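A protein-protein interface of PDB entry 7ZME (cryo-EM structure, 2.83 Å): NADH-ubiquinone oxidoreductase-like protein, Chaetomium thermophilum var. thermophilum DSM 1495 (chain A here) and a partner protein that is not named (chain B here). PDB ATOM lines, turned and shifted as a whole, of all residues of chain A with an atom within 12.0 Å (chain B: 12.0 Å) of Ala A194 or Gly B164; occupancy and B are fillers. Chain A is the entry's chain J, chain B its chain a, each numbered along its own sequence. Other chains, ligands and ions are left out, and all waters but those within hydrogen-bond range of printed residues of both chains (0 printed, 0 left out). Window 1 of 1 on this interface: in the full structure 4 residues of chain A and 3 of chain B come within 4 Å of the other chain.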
ATOM      1  N   ASN A 190       7.362  -6.613 -13.176  1.00  0.00           N
ATOM      2  CA  ASN A 190       6.026  -6.840 -12.634  1.00  0.00           C
ATOM      3  C   ASN A 190       5.053  -7.413 -13.667  1.00  0.00           C
ATOM      4  O   ASN A 190       4.260  -6.681 -14.270  1.00  0.00           O
ATOM      5  CB  ASN A 190       5.514  -5.547 -11.979  1.00  0.00           C
ATOM      6  CG  ASN A 190       5.359  -4.379 -12.957  1.00  0.00           C
ATOM      7  OD1 ASN A 190       5.518  -4.520 -14.168  1.00  0.00           O
ATOM      8  ND2 ASN A 190       5.039  -3.212 -12.414  1.00  0.00           N
ATOM      9  N   PRO A 191       5.071  -8.730 -13.875  1.00  0.00           N
ATOM     10  CA  PRO A 191       4.144  -9.342 -14.835  1.00  0.00           C
ATOM     11  C   PRO A 191       2.690  -9.044 -14.496  1.00  0.00           C
ATOM     12  O   PRO A 191       2.320  -8.880 -13.330  1.00  0.00           O
ATOM     13  CB  PRO A 191       4.440 -10.842 -14.714  1.00  0.00           C
ATOM     14  CG  PRO A 191       5.700 -10.966 -13.909  1.00  0.00           C
ATOM     15  CD  PRO A 191       6.216  -9.606 -13.585  1.00  0.00           C
ATOM     16  N   VAL A 192       1.860  -8.979 -15.538  1.00  0.00           N
ATOM     17  CA  VAL A 192       0.455  -8.604 -15.403  1.00  0.00           C
ATOM     18  C   VAL A 192      -0.318  -9.633 -14.590  1.00  0.00           C
ATOM     19  O   VAL A 192       0.155 -10.753 -14.364  1.00  0.00           O
ATOM     20  CB  VAL A 192      -0.199  -8.403 -16.782  1.00  0.00           C
ATOM     21  CG1 VAL A 192       0.418  -7.212 -17.490  1.00  0.00           C
ATOM     22  CG2 VAL A 192      -0.059  -9.664 -17.626  1.00  0.00           C
ATOM     23  N   CYS A 193      -1.519  -9.257 -14.155  1.00  0.00           N
ATOM     24  CA  CYS A 193      -2.333 -10.069 -13.261  1.00  0.00           C
ATOM     25  C   CYS A 193      -3.254 -11.034 -14.001  1.00  0.00           C
ATOM     26  O   CYS A 193      -4.080 -11.687 -13.359  1.00  0.00           O
ATOM     27  CB  CYS A 193      -3.156  -9.156 -12.340  1.00  0.00           C
ATOM     28  SG  CYS A 193      -3.902  -9.957 -10.894  1.00  0.00           S
ATOM     29  N   ALA A 194      -3.194 -11.069 -15.335  1.00  0.00           N
ATOM     30  CA  ALA A 194      -3.704 -12.165 -16.161  1.00  0.00           C
ATOM     31  C   ALA A 194      -5.071 -12.698 -15.749  1.00  0.00           C
ATOM     32  O   ALA A 194      -5.388 -13.863 -16.015  1.00  0.00           O
ATOM     33  CB  ALA A 194      -2.696 -13.316 -16.180  1.00  0.00           C
ATOM     34  N   ASP A 195      -5.893 -11.863 -15.118  1.00  0.00           N
ATOM     35  CA  ASP A 195      -7.192 -12.298 -14.621  1.00  0.00           C
ATOM     36  C   ASP A 195      -8.035 -11.085 -14.246  1.00  0.00           C
ATOM     37  O   ASP A 195      -7.566 -10.211 -13.506  1.00  0.00           O
ATOM     38  CB  ASP A 195      -7.020 -13.227 -13.416  1.00  0.00           C
ATOM     39  CG  ASP A 195      -8.338 -13.596 -12.767  1.00  0.00           C
ATOM     40  OD1 ASP A 195      -9.324 -13.824 -13.497  1.00  0.00           O
ATOM     41  OD2 ASP A 195      -8.390 -13.658 -11.520  1.00  0.00           O
ATOM     42  N   PRO A 196      -9.273 -10.989 -14.739  1.00  0.00           N
ATOM     43  CA  PRO A 196     -10.131  -9.864 -14.329  1.00  0.00           C
ATOM     44  C   PRO A 196     -10.362  -9.796 -12.830  1.00  0.00           C
ATOM     45  O   PRO A 196     -10.431  -8.698 -12.267  1.00  0.00           O
ATOM     46  CB  PRO A 196     -11.432 -10.127 -15.098  1.00  0.00           C
ATOM     47  CG  PRO A 196     -11.008 -10.926 -16.279  1.00  0.00           C
ATOM     48  CD  PRO A 196      -9.896 -11.803 -15.795  1.00  0.00           C
ATOM     49  N   ASP A 197     -10.483 -10.943 -12.166  1.00  0.00           N
ATOM     50  CA  ASP A 197     -10.648 -10.950 -10.722  1.00  0.00           C
ATOM     51  C   ASP A 197      -9.309 -10.709 -10.030  1.00  0.00           C
ATOM     52  O   ASP A 197      -8.239 -10.785 -10.641  1.00  0.00           O
ATOM     53  CB  ASP A 197     -11.251 -12.275 -10.255  1.00  0.00           C
ATOM     54  N   GLN A 198      -9.385 -10.413  -8.734  1.00  0.00           N
ATOM     55  CA  GLN A 198      -8.208 -10.159  -7.904  1.00  0.00           C
ATOM     56  C   GLN A 198      -7.341  -9.040  -8.474  1.00  0.00           C
ATOM     57  O   GLN A 198      -7.670  -7.861  -8.342  1.00  0.00           O
ATOM     58  CB  GLN A 198      -7.377 -11.435  -7.743  1.00  0.00           C
ATOM     59  N   GLY B 154     -16.263   2.705 -18.644  1.00  0.00           N
ATOM     60  CA  GLY B 154     -15.374   1.865 -17.875  1.00  0.00           C
ATOM     61  C   GLY B 154     -14.147   1.393 -18.619  1.00  0.00           C
ATOM     62  O   GLY B 154     -13.361   0.619 -18.056  1.00  0.00           O
ATOM     63  N   GLY B 155     -13.954   1.831 -19.861  1.00  0.00           N
ATOM     64  CA  GLY B 155     -12.793   1.431 -20.628  1.00  0.00           C
ATOM     65  C   GLY B 155     -12.753  -0.028 -21.004  1.00  0.00           C
ATOM     66  O   GLY B 155     -11.680  -0.540 -21.326  1.00  0.00           O
ATOM     67  N   LEU B 156     -13.898  -0.713 -20.979  1.00  0.00           N
ATOM     68  CA  LEU B 156     -13.963  -2.148 -21.264  1.00  0.00           C
ATOM     69  C   LEU B 156     -13.003  -2.916 -20.362  1.00  0.00           C
ATOM     70  O   LEU B 156     -12.304  -3.830 -20.798  1.00  0.00           O
ATOM     71  CB  LEU B 156     -13.674  -2.426 -22.740  1.00  0.00           C
ATOM     72  CG  LEU B 156     -14.786  -2.372 -23.790  1.00  0.00           C
ATOM     73  CD1 LEU B 156     -15.773  -3.484 -23.586  1.00  0.00           C
ATOM     74  CD2 LEU B 156     -15.503  -1.049 -23.743  1.00  0.00           C
ATOM     75  N   GLU B 157     -12.971  -2.532 -19.086  1.00  0.00           N
ATOM     76  CA  GLU B 157     -11.944  -3.024 -18.173  1.00  0.00           C
ATOM     77  C   GLU B 157     -12.028  -4.536 -17.997  1.00  0.00           C
ATOM     78  O   GLU B 157     -11.092  -5.267 -18.340  1.00  0.00           O
ATOM     79  CB  GLU B 157     -12.073  -2.314 -16.824  1.00  0.00           C
ATOM     80  CG  GLU B 157     -11.026  -2.713 -15.799  1.00  0.00           C
ATOM     81  CD  GLU B 157      -9.624  -2.310 -16.208  1.00  0.00           C
ATOM     82  OE1 GLU B 157      -9.481  -1.340 -16.982  1.00  0.00           O
ATOM     83  OE2 GLU B 157      -8.662  -2.961 -15.751  1.00  0.00           O
ATOM     84  N   ARG B 158     -13.148  -5.023 -17.462  1.00  0.00           N
ATOM     85  CA  ARG B 158     -13.251  -6.438 -17.120  1.00  0.00           C
ATOM     86  C   ARG B 158     -13.241  -7.317 -18.364  1.00  0.00           C
ATOM     87  O   ARG B 158     -12.500  -8.306 -18.431  1.00  0.00           O
ATOM     88  CB  ARG B 158     -14.518  -6.684 -16.301  1.00  0.00           C
ATOM     89  CG  ARG B 158     -14.629  -5.823 -15.055  1.00  0.00           C
ATOM     90  CD  ARG B 158     -15.728  -6.327 -14.134  1.00  0.00           C
ATOM     91  NE  ARG B 158     -17.052  -5.908 -14.582  1.00  0.00           N
ATOM     92  CZ  ARG B 158     -17.969  -6.734 -15.075  1.00  0.00           C
ATOM     93  NH1 ARG B 158     -19.149  -6.266 -15.457  1.00  0.00           N
ATOM     94  NH2 ARG B 158     -17.707  -8.028 -15.186  1.00  0.00           N
ATOM     95  N   GLU B 159     -14.043  -6.967 -19.363  1.00  0.00           N
ATOM     96  CA  GLU B 159     -14.303  -7.849 -20.494  1.00  0.00           C
ATOM     97  C   GLU B 159     -13.267  -7.747 -21.606  1.00  0.00           C
ATOM     98  O   GLU B 159     -13.399  -8.447 -22.614  1.00  0.00           O
ATOM     99  CB  GLU B 159     -15.710  -7.594 -21.050  1.00  0.00           C
ATOM    100  CG  GLU B 159     -15.998  -6.170 -21.473  1.00  0.00           C
ATOM    101  CD  GLU B 159     -16.280  -5.243 -20.301  1.00  0.00           C
ATOM    102  OE1 GLU B 159     -16.569  -4.051 -20.537  1.00  0.00           O
ATOM    103  OE2 GLU B 159     -16.221  -5.704 -19.142  1.00  0.00           O
ATOM    104  N   LEU B 160     -12.239  -6.914 -21.452  1.00  0.00           N
ATOM    105  CA  LEU B 160     -11.077  -6.962 -22.327  1.00  0.00           C
ATOM    106  C   LEU B 160      -9.895  -7.663 -21.676  1.00  0.00           C
ATOM    107  O   LEU B 160      -8.770  -7.560 -22.173  1.00  0.00           O
ATOM    108  CB  LEU B 160     -10.673  -5.558 -22.776  1.00  0.00           C
ATOM    109  CG  LEU B 160     -11.434  -5.006 -23.977  1.00  0.00           C
ATOM    110  CD1 LEU B 160     -10.850  -3.680 -24.400  1.00  0.00           C
ATOM    111  CD2 LEU B 160     -11.376  -5.998 -25.114  1.00  0.00           C
ATOM    112  N   GLY B 161     -10.126  -8.373 -20.579  1.00  0.00           N
ATOM    113  CA  GLY B 161      -9.085  -9.126 -19.919  1.00  0.00           C
ATOM    114  C   GLY B 161      -8.646  -8.607 -18.571  1.00  0.00           C
ATOM    115  O   GLY B 161      -7.672  -9.126 -18.018  1.00  0.00           O
ATOM    116  N   GLY B 162      -9.323  -7.607 -18.020  1.00  0.00           N
ATOM    117  CA  GLY B 162      -8.931  -7.060 -16.744  1.00  0.00           C
ATOM    118  C   GLY B 162      -7.752  -6.114 -16.865  1.00  0.00           C
ATOM    119  O   GLY B 162      -7.325  -5.725 -17.954  1.00  0.00           O
ATOM    120  N   ALA B 163      -7.220  -5.738 -15.699  1.00  0.00           N
ATOM    121  CA  ALA B 163      -6.076  -4.835 -15.654  1.00  0.00           C
ATOM    122  C   ALA B 163      -4.822  -5.459 -16.248  1.00  0.00           C
ATOM    123  O   ALA B 163      -3.890  -4.728 -16.599  1.00  0.00           O
ATOM    124  CB  ALA B 163      -5.808  -4.397 -14.215  1.00  0.00           C
ATOM    125  N   GLY B 164      -4.779  -6.783 -16.371  1.00  0.00           N
ATOM    126  CA  GLY B 164      -3.644  -7.465 -16.950  1.00  0.00           C
ATOM    127  C   GLY B 164      -3.568  -7.433 -18.457  1.00  0.00           C
ATOM    128  O   GLY B 164      -2.576  -7.889 -19.029  1.00  0.00           O
ATOM    129  N   ALA B 165      -4.590  -6.903 -19.120  1.00  0.00           N
ATOM    130  CA  ALA B 165      -4.609  -6.781 -20.567  1.00  0.00           C
ATOM    131  C   ALA B 165      -4.866  -5.328 -20.941  1.00  0.00           C
ATOM    132  O   ALA B 165      -5.119  -4.478 -20.085  1.00  0.00           O
ATOM    133  CB  ALA B 165      -5.668  -7.699 -21.192  1.00  0.00           C
ATOM    134  N   VAL B 166      -4.793  -5.045 -22.242  1.00  0.00           N
ATOM    135  CA  VAL B 166      -5.022  -3.690 -22.723  1.00  0.00           C
ATOM    136  C   VAL B 166      -6.507  -3.360 -22.636  1.00  0.00           C
ATOM    137  O   VAL B 166      -7.371  -4.220 -22.855  1.00  0.00           O
ATOM    138  CB  VAL B 166      -4.485  -3.528 -24.157  1.00  0.00           C
ATOM    139  CG1 VAL B 166      -5.274  -4.387 -25.133  1.00  0.00           C
ATOM    140  CG2 VAL B 166      -4.508  -2.066 -24.578  1.00  0.00           C
ATOM    141  N   ARG B 167      -6.809  -2.113 -22.293  1.00  0.00           N
ATOM    142  CA  ARG B 167      -8.173  -1.631 -22.143  1.00  0.00           C
ATOM    143  C   ARG B 167      -8.538  -0.739 -23.324  1.00  0.00           C
ATOM    144  O   ARG B 167      -7.732  -0.495 -24.225  1.00  0.00           O
ATOM    145  CB  ARG B 167      -8.335  -0.882 -20.819  1.00  0.00           C
ATOM    146  CG  ARG B 167      -7.386   0.293 -20.656  1.00  0.00           C
ATOM    147  CD  ARG B 167      -7.184   0.644 -19.193  1.00  0.00           C
ATOM    148  NE  ARG B 167      -8.114   1.676 -18.745  1.00  0.00           N
ATOM    149  CZ  ARG B 167      -7.874   2.981 -18.814  1.00  0.00           C
ATOM    150  NH1 ARG B 167      -6.727   3.418 -19.317  1.00  0.00           N
ATOM    151  NH2 ARG B 167      -8.778   3.848 -18.382  1.00  0.00           N
ATOM    152  N   ALA B 168      -9.770  -0.247 -23.307  1.00  0.00           N
ATOM    153  CA  ALA B 168     -10.291   0.611 -24.354  1.00  0.00           C
ATOM    154  C   ALA B 168     -10.144   2.078 -23.949  1.00  0.00           C
ATOM    155  O   ALA B 168      -9.507   2.411 -22.945  1.00  0.00           O
ATOM    156  CB  ALA B 168     -11.742   0.233 -24.653  1.00  0.00           C
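The backbone NH (N) of Gly B162 is in hydrogen-bond range of the backbone carbonyl oxygen (O) of Glu B157 (3.0 Å).
Among the printed residues, merely in contact across the chains: Val A192 with Gly B164, Pro A196 with Arg B158, Pro A196 with Gly B162, Cys A193 with Gly B164 and Ala A194 with Gly B164.
Gly B164 touches just these residues of chain A: Val A192, Cys A193 and Ala A194. Of chain B, only Gly B164 (3.9 Å) comes within 4 Å of Cys A193. No residue of chain B comes within 4 Å of Asp A195. No residue of chain A comes within 4 Å of Gly B161. No residue of chain A comes within 4 Å of Ala B163. No residue of chain A comes within 4 Å of Ala B165. Printed residues of chain A within 4 Å of Arg B158: Pro A196. Arg B167 touches none of the printed residues of chain A. Gly B154 touches none of the printed residues of chain A. The nearest printed residue of chain A that does not touch Arg B158 is Asp A195 (6.7 Å).
Printed residues of chain B that touch a printed residue of chain A: Arg B158, Gly B162 and Gly B164. Hydrophobic or aromatic side chains of chain A that line the printed part of chain B: Val A192 and Pro A196. Among the printed residues, 5 pairs touch across the chains.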
